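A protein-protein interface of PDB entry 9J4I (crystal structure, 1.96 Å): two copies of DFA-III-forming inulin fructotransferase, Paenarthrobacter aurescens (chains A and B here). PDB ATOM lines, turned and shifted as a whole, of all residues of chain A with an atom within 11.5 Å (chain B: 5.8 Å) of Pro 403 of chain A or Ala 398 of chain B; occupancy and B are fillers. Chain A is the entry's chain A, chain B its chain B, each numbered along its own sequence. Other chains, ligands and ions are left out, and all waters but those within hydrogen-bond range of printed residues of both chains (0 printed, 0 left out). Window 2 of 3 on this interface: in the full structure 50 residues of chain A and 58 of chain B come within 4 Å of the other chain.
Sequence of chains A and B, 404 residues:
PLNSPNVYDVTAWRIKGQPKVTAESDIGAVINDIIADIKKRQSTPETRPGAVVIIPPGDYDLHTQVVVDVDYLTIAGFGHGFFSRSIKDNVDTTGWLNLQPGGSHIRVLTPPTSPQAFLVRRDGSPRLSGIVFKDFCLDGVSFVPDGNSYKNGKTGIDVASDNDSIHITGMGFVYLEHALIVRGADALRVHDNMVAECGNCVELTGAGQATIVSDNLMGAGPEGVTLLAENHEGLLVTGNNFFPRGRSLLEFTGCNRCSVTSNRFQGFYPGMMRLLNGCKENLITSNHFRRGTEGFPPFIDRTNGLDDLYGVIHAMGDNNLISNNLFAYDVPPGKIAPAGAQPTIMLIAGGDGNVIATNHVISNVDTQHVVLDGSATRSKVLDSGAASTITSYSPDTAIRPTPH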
ATOM      1  N   ALA A 357      -1.609 -17.957  21.346  1.00  0.00           N
ATOM      2  CA  ALA A 357      -1.693 -18.125  19.881  1.00  0.00           C
ATOM      3  C   ALA A 357      -1.914 -16.783  19.190  1.00  0.00           C
ATOM      4  O   ALA A 357      -2.883 -16.091  19.528  1.00  0.00           O
ATOM      5  CB  ALA A 357      -2.803 -19.109  19.556  1.00  0.00           C
ATOM      6  N   THR A 358      -1.085 -16.486  18.190  1.00  0.00           N
ATOM      7  CA  THR A 358      -1.289 -15.390  17.219  1.00  0.00           C
ATOM      8  C   THR A 358      -1.301 -14.056  17.962  1.00  0.00           C
ATOM      9  O   THR A 358      -2.224 -13.261  17.773  1.00  0.00           O
ATOM     10  CB  THR A 358      -2.580 -15.559  16.403  1.00  0.00           C
ATOM     11  OG1 THR A 358      -2.803 -16.954  16.211  1.00  0.00           O
ATOM     12  CG2 THR A 358      -2.499 -14.835  15.076  1.00  0.00           C
ATOM     13  N   ASN A 359      -0.291 -13.819  18.781  1.00  0.00           N
ATOM     14  CA  ASN A 359      -0.148 -12.548  19.515  1.00  0.00           C
ATOM     15  C   ASN A 359       0.982 -11.750  18.865  1.00  0.00           C
ATOM     16  O   ASN A 359       2.049 -12.336  18.598  1.00  0.00           O
ATOM     17  CB  ASN A 359       0.068 -12.811  20.998  1.00  0.00           C
ATOM     18  CG  ASN A 359      -1.154 -13.451  21.608  1.00  0.00           C
ATOM     19  OD1 ASN A 359      -2.148 -12.772  21.836  1.00  0.00           O
ATOM     20  ND2 ASN A 359      -1.064 -14.732  21.917  1.00  0.00           N
ATOM     21  N   HIS A 360       0.755 -10.466  18.599  1.00  0.00           N
ATOM     22  CA  HIS A 360       1.820  -9.580  18.061  1.00  0.00           C
ATOM     23  C   HIS A 360       2.341  -8.689  19.194  1.00  0.00           C
ATOM     24  O   HIS A 360       1.558  -7.922  19.796  1.00  0.00           O
ATOM     25  CB  HIS A 360       1.348  -8.818  16.825  1.00  0.00           C
ATOM     26  CG  HIS A 360       2.447  -8.001  16.235  1.00  0.00           C
ATOM     27  ND1 HIS A 360       3.722  -8.517  16.048  1.00  0.00           N
ATOM     28  CD2 HIS A 360       2.490  -6.711  15.846  1.00  0.00           C
ATOM     29  CE1 HIS A 360       4.502  -7.566  15.560  1.00  0.00           C
ATOM     30  NE2 HIS A 360       3.769  -6.454  15.429  1.00  0.00           N
ATOM     31  N   HIS A 369       8.295 -12.528  24.999  1.00  0.00           N
ATOM     32  CA  HIS A 369       6.868 -12.409  24.596  1.00  0.00           C
ATOM     33  C   HIS A 369       6.054 -13.312  25.518  1.00  0.00           C
ATOM     34  O   HIS A 369       4.966 -12.901  25.963  1.00  0.00           O
ATOM     35  CB  HIS A 369       6.693 -12.788  23.119  1.00  0.00           C
ATOM     36  CG  HIS A 369       7.255 -11.821  22.130  1.00  0.00           C
ATOM     37  ND1 HIS A 369       6.881 -11.847  20.790  1.00  0.00           N
ATOM     38  CD2 HIS A 369       8.154 -10.811  22.261  1.00  0.00           C
ATOM     39  CE1 HIS A 369       7.515 -10.883  20.138  1.00  0.00           C
ATOM     40  NE2 HIS A 369       8.321 -10.247  21.021  1.00  0.00           N
ATOM     41  N   VAL A 381       2.361 -22.729  22.690  1.00  0.00           N
ATOM     42  CA  VAL A 381       2.685 -21.356  22.237  1.00  0.00           C
ATOM     43  C   VAL A 381       2.833 -21.407  20.724  1.00  0.00           C
ATOM     44  O   VAL A 381       3.774 -22.067  20.240  1.00  0.00           O
ATOM     45  CB  VAL A 381       3.940 -20.780  22.916  1.00  0.00           C
ATOM     46  CG1 VAL A 381       4.152 -19.337  22.484  1.00  0.00           C
ATOM     47  CG2 VAL A 381       3.856 -20.895  24.432  1.00  0.00           C
ATOM     48  N   LEU A 382       1.950 -20.693  20.037  1.00  0.00           N
ATOM     49  CA  LEU A 382       1.873 -20.634  18.557  1.00  0.00           C
ATOM     50  C   LEU A 382       1.971 -19.184  18.100  1.00  0.00           C
ATOM     51  O   LEU A 382       1.204 -18.327  18.596  1.00  0.00           O
ATOM     52  CB  LEU A 382       0.551 -21.246  18.106  1.00  0.00           C
ATOM     53  CG  LEU A 382       0.176 -22.568  18.769  1.00  0.00           C
ATOM     54  CD1 LEU A 382      -1.179 -23.024  18.256  1.00  0.00           C
ATOM     55  CD2 LEU A 382       1.225 -23.634  18.509  1.00  0.00           C
ATOM     56  N   ASP A 383       2.923 -18.901  17.224  1.00  0.00           N
ATOM     57  CA  ASP A 383       2.927 -17.653  16.423  1.00  0.00           C
ATOM     58  C   ASP A 383       2.799 -16.427  17.338  1.00  0.00           C
ATOM     59  O   ASP A 383       2.026 -15.497  16.999  1.00  0.00           O
ATOM     60  CB  ASP A 383       1.798 -17.713  15.397  1.00  0.00           C
ATOM     61  CG  ASP A 383       1.905 -18.925  14.493  1.00  0.00           C
ATOM     62  OD1 ASP A 383       3.038 -19.363  14.218  1.00  0.00           O
ATOM     63  OD2 ASP A 383       0.860 -19.438  14.097  1.00  0.00           O
ATOM     64  N   SER A 384       3.517 -16.417  18.464  1.00  0.00           N
ATOM     65  CA  SER A 384       3.473 -15.296  19.439  1.00  0.00           C
ATOM     66  C   SER A 384       4.887 -14.753  19.673  1.00  0.00           C
ATOM     67  O   SER A 384       5.093 -14.070  20.706  1.00  0.00           O
ATOM     68  CB  SER A 384       2.782 -15.713  20.708  1.00  0.00           C
ATOM     69  OG  SER A 384       1.451 -16.148  20.439  1.00  0.00           O
ATOM     70  N   GLY A 385       5.777 -14.975  18.696  1.00  0.00           N
ATOM     71  CA  GLY A 385       7.159 -14.456  18.660  1.00  0.00           C
ATOM     72  C   GLY A 385       8.148 -15.466  18.091  1.00  0.00           C
ATOM     73  O   GLY A 385       7.847 -16.691  18.093  1.00  0.00           O
ATOM     74  N   ALA A 386       9.319 -14.990  17.657  1.00  0.00           N
ATOM     75  CA  ALA A 386      10.483 -15.839  17.304  1.00  0.00           C
ATOM     76  C   ALA A 386      10.874 -16.693  18.523  1.00  0.00           C
ATOM     77  O   ALA A 386      10.503 -16.334  19.659  1.00  0.00           O
ATOM     78  CB  ALA A 386      11.631 -14.980  16.826  1.00  0.00           C
ATOM     79  N   ALA A 387      11.611 -17.781  18.305  1.00  0.00           N
ATOM     80  CA  ALA A 387      12.021 -18.751  19.352  1.00  0.00           C
ATOM     81  C   ALA A 387      12.757 -18.025  20.490  1.00  0.00           C
ATOM     82  O   ALA A 387      12.611 -18.448  21.648  1.00  0.00           O
ATOM     83  CB  ALA A 387      12.879 -19.833  18.744  1.00  0.00           C
ATOM     84  N   SER A 388      13.520 -16.977  20.168  1.00  0.00           N
ATOM     85  CA  SER A 388      14.380 -16.227  21.121  1.00  0.00           C
ATOM     86  C   SER A 388      13.515 -15.360  22.050  1.00  0.00           C
ATOM     87  O   SER A 388      14.053 -14.835  23.033  1.00  0.00           O
ATOM     88  CB  SER A 388      15.407 -15.389  20.386  1.00  0.00           C
ATOM     89  OG  SER A 388      14.794 -14.557  19.411  1.00  0.00           O
ATOM     90  N   THR A 389      12.228 -15.191  21.742  1.00  0.00           N
ATOM     91  CA  THR A 389      11.266 -14.403  22.560  1.00  0.00           C
ATOM     92  C   THR A 389      10.347 -15.320  23.379  1.00  0.00           C
ATOM     93  O   THR A 389       9.555 -14.779  24.162  1.00  0.00           O
ATOM     94  CB  THR A 389      10.479 -13.457  21.652  1.00  0.00           C
ATOM     95  OG1 THR A 389       9.510 -14.214  20.921  1.00  0.00           O
ATOM     96  CG2 THR A 389      11.387 -12.684  20.720  1.00  0.00           C
ATOM     97  N   ILE A 390      10.421 -16.650  23.217  1.00  0.00           N
ATOM     98  CA  ILE A 390       9.604 -17.600  24.032  1.00  0.00           C
ATOM     99  C   ILE A 390      10.539 -18.349  24.981  1.00  0.00           C
ATOM    100  O   ILE A 390      11.454 -19.002  24.481  1.00  0.00           O
ATOM    101  CB  ILE A 390       8.819 -18.591  23.149  1.00  0.00           C
ATOM    102  CG1 ILE A 390       8.133 -17.898  21.972  1.00  0.00           C
ATOM    103  CG2 ILE A 390       7.841 -19.413  23.984  1.00  0.00           C
ATOM    104  CD1 ILE A 390       7.212 -16.766  22.368  1.00  0.00           C
ATOM    105  N   ILE A 399       6.033 -25.324  21.225  1.00  0.00           N
ATOM    106  CA  ILE A 399       6.272 -23.943  20.733  1.00  0.00           C
ATOM    107  C   ILE A 399       6.380 -23.995  19.214  1.00  0.00           C
ATOM    108  O   ILE A 399       7.228 -24.730  18.702  1.00  0.00           O
ATOM    109  CB  ILE A 399       7.551 -23.314  21.337  1.00  0.00           C
ATOM    110  CG1 ILE A 399       7.497 -23.232  22.866  1.00  0.00           C
ATOM    111  CG2 ILE A 399       7.808 -21.952  20.703  1.00  0.00           C
ATOM    112  CD1 ILE A 399       8.867 -23.079  23.532  1.00  0.00           C
ATOM    113  N   ARG A 400       5.567 -23.213  18.527  1.00  0.00           N
ATOM    114  CA  ARG A 400       5.783 -22.895  17.103  1.00  0.00           C
ATOM    115  C   ARG A 400       6.175 -21.424  17.042  1.00  0.00           C
ATOM    116  O   ARG A 400       5.363 -20.546  17.360  1.00  0.00           O
ATOM    117  CB  ARG A 400       4.563 -23.216  16.237  1.00  0.00           C
ATOM    118  CG  ARG A 400       4.755 -22.820  14.780  1.00  0.00           C
ATOM    119  CD  ARG A 400       3.626 -23.247  13.859  1.00  0.00           C
ATOM    120  NE  ARG A 400       2.435 -22.449  14.105  1.00  0.00           N
ATOM    121  CZ  ARG A 400       1.198 -22.930  14.293  1.00  0.00           C
ATOM    122  NH1 ARG A 400       0.949 -24.227  14.272  1.00  0.00           N
ATOM    123  NH2 ARG A 400       0.209 -22.083  14.493  1.00  0.00           N
ATOM    124  N   PRO A 401       7.440 -21.128  16.657  1.00  0.00           N
ATOM    125  CA  PRO A 401       7.893 -19.753  16.507  1.00  0.00           C
ATOM    126  C   PRO A 401       7.149 -19.115  15.333  1.00  0.00           C
ATOM    127  O   PRO A 401       6.799 -19.806  14.371  1.00  0.00           O
ATOM    128  CB  PRO A 401       9.409 -19.844  16.232  1.00  0.00           C
ATOM    129  CG  PRO A 401       9.784 -21.293  16.491  1.00  0.00           C
ATOM    130  CD  PRO A 401       8.506 -22.100  16.347  1.00  0.00           C
ATOM    131  N   THR A 402       6.909 -17.814  15.430  1.00  0.00           N
ATOM    132  CA  THR A 402       6.479 -16.992  14.281  1.00  0.00           C
ATOM    133  C   THR A 402       7.501 -17.213  13.169  1.00  0.00           C
ATOM    134  O   THR A 402       8.691 -17.082  13.406  1.00  0.00           O
ATOM    135  CB  THR A 402       6.347 -15.522  14.669  1.00  0.00           C
ATOM    136  OG1 THR A 402       5.478 -15.458  15.804  1.00  0.00           O
ATOM    137  CG2 THR A 402       5.814 -14.692  13.525  1.00  0.00           C
ATOM    138  N   PRO A 403       7.067 -17.569  11.944  1.00  0.00           N
ATOM    139  CA  PRO A 403       7.976 -17.794  10.810  1.00  0.00           C
ATOM    140  C   PRO A 403       9.060 -16.729  10.569  1.00  0.00           C
ATOM    141  O   PRO A 403       8.655 -15.576  10.771  1.00  0.00           O
ATOM    142  CB  PRO A 403       6.981 -17.760   9.644  1.00  0.00           C
ATOM    143  CG  PRO A 403       5.754 -18.418  10.222  1.00  0.00           C
ATOM    144  CD  PRO A 403       5.654 -17.818  11.601  1.00  0.00           C
ATOM    145  N   SER B 379       7.880  -7.783   7.268  1.00  0.00           N
ATOM    146  CA  SER B 379       6.446  -8.168   7.207  1.00  0.00           C
ATOM    147  C   SER B 379       6.286  -9.672   7.499  1.00  0.00           C
ATOM    148  O   SER B 379       7.224 -10.443   7.196  1.00  0.00           O
ATOM    149  CB  SER B 379       5.869  -7.780   5.897  1.00  0.00           C
ATOM    150  OG  SER B 379       6.068  -6.395   5.658  1.00  0.00           O
ATOM    151  N   LYS B 380       5.161 -10.073   8.112  1.00  0.00           N
ATOM    152  CA  LYS B 380       4.795 -11.502   8.344  1.00  0.00           C
ATOM    153  C   LYS B 380       3.411 -11.742   7.741  1.00  0.00           C
ATOM    154  O   LYS B 380       2.493 -10.929   8.009  1.00  0.00           O
ATOM    155  CB  LYS B 380       4.728 -11.869   9.827  1.00  0.00           C
ATOM    156  CG  LYS B 380       5.942 -11.483  10.666  1.00  0.00           C
ATOM    157  CD  LYS B 380       7.121 -12.325  10.381  1.00  0.00           C
ATOM    158  CE  LYS B 380       8.310 -11.955  11.240  1.00  0.00           C
ATOM    159  NZ  LYS B 380       9.441 -12.868  10.951  1.00  0.00           N
ATOM    160  N   VAL B 381       3.255 -12.782   6.928  1.00  0.00           N
ATOM    161  CA  VAL B 381       1.917 -13.174   6.395  1.00  0.00           C
ATOM    162  C   VAL B 381       1.713 -14.649   6.742  1.00  0.00           C
ATOM    163  O   VAL B 381       2.516 -15.456   6.240  1.00  0.00           O
ATOM    164  CB  VAL B 381       1.778 -12.916   4.885  1.00  0.00           C
ATOM    165  CG1 VAL B 381       0.408 -13.308   4.366  1.00  0.00           C
ATOM    166  CG2 VAL B 381       2.055 -11.472   4.527  1.00  0.00           C
ATOM    167  N   LEU B 382       0.735 -14.958   7.608  1.00  0.00           N
ATOM    168  CA  LEU B 382       0.465 -16.331   8.102  1.00  0.00           C
ATOM    169  C   LEU B 382      -0.986 -16.685   7.766  1.00  0.00           C
ATOM    170  O   LEU B 382      -1.877 -15.873   8.086  1.00  0.00           O
ATOM    171  CB  LEU B 382       0.682 -16.444   9.618  1.00  0.00           C
ATOM    172  CG  LEU B 382       1.783 -15.615  10.268  1.00  0.00           C
ATOM    173  CD1 LEU B 382       1.815 -15.923  11.762  1.00  0.00           C
ATOM    174  CD2 LEU B 382       3.144 -15.884   9.636  1.00  0.00           C
ATOM    175  N   ASP B 396      11.940  -9.255   1.870  1.00  0.00           N
ATOM    176  CA  ASP B 396      12.194  -9.771   3.242  1.00  0.00           C
ATOM    177  C   ASP B 396      10.894 -10.203   3.947  1.00  0.00           C
ATOM    178  O   ASP B 396      10.954 -10.452   5.146  1.00  0.00           O
ATOM    179  CB  ASP B 396      12.981  -8.750   4.069  1.00  0.00           C
ATOM    180  CG  ASP B 396      12.182  -7.532   4.502  1.00  0.00           C
ATOM    181  OD1 ASP B 396      11.252  -7.129   3.760  1.00  0.00           O
ATOM    182  OD2 ASP B 396      12.495  -7.009   5.591  1.00  0.00           O
ATOM    183  N   THR B 397       9.777 -10.357   3.240  1.00  0.00           N
ATOM    184  CA  THR B 397       8.498 -10.811   3.846  1.00  0.00           C
ATOM    185  C   THR B 397       8.591 -12.305   4.191  1.00  0.00           C
ATOM    186  O   THR B 397       8.891 -13.097   3.266  1.00  0.00           O
ATOM    187  CB  THR B 397       7.319 -10.583   2.900  1.00  0.00           C
ATOM    188  OG1 THR B 397       7.209  -9.188   2.610  1.00  0.00           O
ATOM    189  CG2 THR B 397       6.009 -11.084   3.467  1.00  0.00           C
ATOM    190  N   ALA B 398       8.286 -12.688   5.435  1.00  0.00           N
ATOM    191  CA  ALA B 398       8.135 -14.113   5.841  1.00  0.00           C
ATOM    192  C   ALA B 398       6.699 -14.564   5.560  1.00  0.00           C
ATOM    193  O   ALA B 398       5.732 -13.900   6.049  1.00  0.00           O
ATOM    194  CB  ALA B 398       8.514 -14.333   7.283  1.00  0.00           C
ATOM    195  N   ILE B 399       6.549 -15.630   4.768  1.00  0.00           N
ATOM    196  CA  ILE B 399       5.215 -16.100   4.282  1.00  0.00           C
ATOM    197  C   ILE B 399       5.015 -17.559   4.699  1.00  0.00           C
ATOM    198  O   ILE B 399       5.813 -18.431   4.285  1.00  0.00           O
ATOM    199  CB  ILE B 399       5.044 -15.892   2.761  1.00  0.00           C
ATOM    200  CG1 ILE B 399       5.262 -14.428   2.367  1.00  0.00           C
ATOM    201  CG2 ILE B 399       3.684 -16.418   2.301  1.00  0.00           C
ATOM    202  CD1 ILE B 399       5.283 -14.174   0.880  1.00  0.00           C
ATOM    203  N   ARG B 400       3.964 -17.814   5.479  1.00  0.00           N
ATOM    204  CA  ARG B 400       3.414 -19.176   5.672  1.00  0.00           C
ATOM    205  C   ARG B 400       2.087 -19.264   4.927  1.00  0.00           C
ATOM    206  O   ARG B 400       1.083 -18.680   5.336  1.00  0.00           O
ATOM    207  CB  ARG B 400       3.249 -19.527   7.150  1.00  0.00           C
ATOM    208  CG  ARG B 400       2.232 -20.636   7.355  1.00  0.00           C
ATOM    209  CD  ARG B 400       2.561 -21.682   8.383  1.00  0.00           C
ATOM    210  NE  ARG B 400       3.098 -21.229   9.642  1.00  0.00           N
ATOM    211  CZ  ARG B 400       2.441 -20.614  10.625  1.00  0.00           C
ATOM    212  NH1 ARG B 400       1.182 -20.249  10.514  1.00  0.00           N
ATOM    213  NH2 ARG B 400       3.089 -20.338  11.732  1.00  0.00           N
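The side-chain amino group (NZ) of Lys 380 of chain B sits at hydrogen-bond distance from the backbone carbonyl oxygen (O) of Pro 403 of chain A. The guanidinium group (NE) of Arg 400 of chain A sits close to the guanidinium group (NH2) of Arg 400 of chain B, 3.2 Å away. The side-chain carboxylate (OD1) of Asp 383 of chain A is in salt-bridge range of the guanidinium group (NH2) of Arg 400 of chain B, 2.7 Å away.
Of the 9 printed residues of chain B, 4 touch a printed residue of chain A. Printed residues of chain B that touch a printed residue of chain A: Lys 380, Leu 382, Ala 398 and Arg 400. Among the printed residues, 6 pairs touch across the chains. Among the printed residues, Asp or Glu carboxylates within 4 Å of a Lys or Arg side-chain nitrogen of the other chain: Asp 383 of chain A with Arg 400 of chain B (2.7 Å).
Ala 357 of chain A touches none of the printed residues of chain B. Asn 359 of chain A touches none of the printed residues of chain B. Of the printed residues of chain B, Asp 383 of chain A touches Arg 400 (2.7 Å). Printed residues of chain B within 4 Å of Pro 403 of chain A: Lys 380, Leu 382, Ala 398 and Arg 400. No residue of chain A comes within 4 Å of Ser 379 of chain B. Of chain A, only Pro 403 (2.8 Å) comes within 4 Å of Lys 380 of chain B. No residue of chain A comes within 4 Å of Val 381 of chain B. Printed residues of chain A within 4 Å of Leu 382 of chain B: Pro 403. No residue of chain A comes within 4 Å of Asp 396 of chain B. Of the printed residues of chain A, Ala 398 of chain B touches Pro 403 (3.7 Å). Arg 400 of chain B touches just these residues of chain A: Asp 383 (2.7 Å), Arg 400 (3.2 Å) and Pro 403 (3.6 Å). The nearest residue of chain B that does not touch Pro 403 of chain A is Ile 399 of chain B (5.3 Å). The nearest residue of chain A that does not touch Ala 398 of chain B is Thr 402 of chain A (6.6 Å). The nearest printed residue of chain B that does not touch Asp 383 of chain A is Leu 382 of chain B (4.1 Å).
The backbone NH of Val 381 of chain B lies within hydrogen-bond range of the backbone carbonyl oxygen of Ala 398 of chain B (2.9 Å). The backbone NH (N) of Thr 358 of chain A sits close to the backbone carbonyl oxygen (O) of Asp 383 of chain A, at 3.5 Å. NH2 of Arg 400 of chain A is in salt-bridge range of OD2 of Asp 383 of chain A, 2.8 Å away. O of Val 381 of chain B sits at hydrogen-bond distance from N of Arg 400 of chain B. The backbone carbonyl oxygen of Ser 379 of chain B sits at hydrogen-bond distance from the backbone NH of Ala 398 of chain B (3.0 Å). The backbone NH (N) of Asn 359 of chain A lies within hydrogen-bond range of the backbone carbonyl oxygen (O) of Asp 383 of chain A, at 3.4 Å.
Among the printed residues, pairs that only touch across the chains: Pro 403 of chain A with Leu 382 of chain B, Pro 403 of chain A with Ala 398 of chain B and Pro 403 of chain A with Arg 400 of chain B.
Arg 400 of chain B touches its own counterpart, Arg 400 of chain A. 4 positions are printed for both chains.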
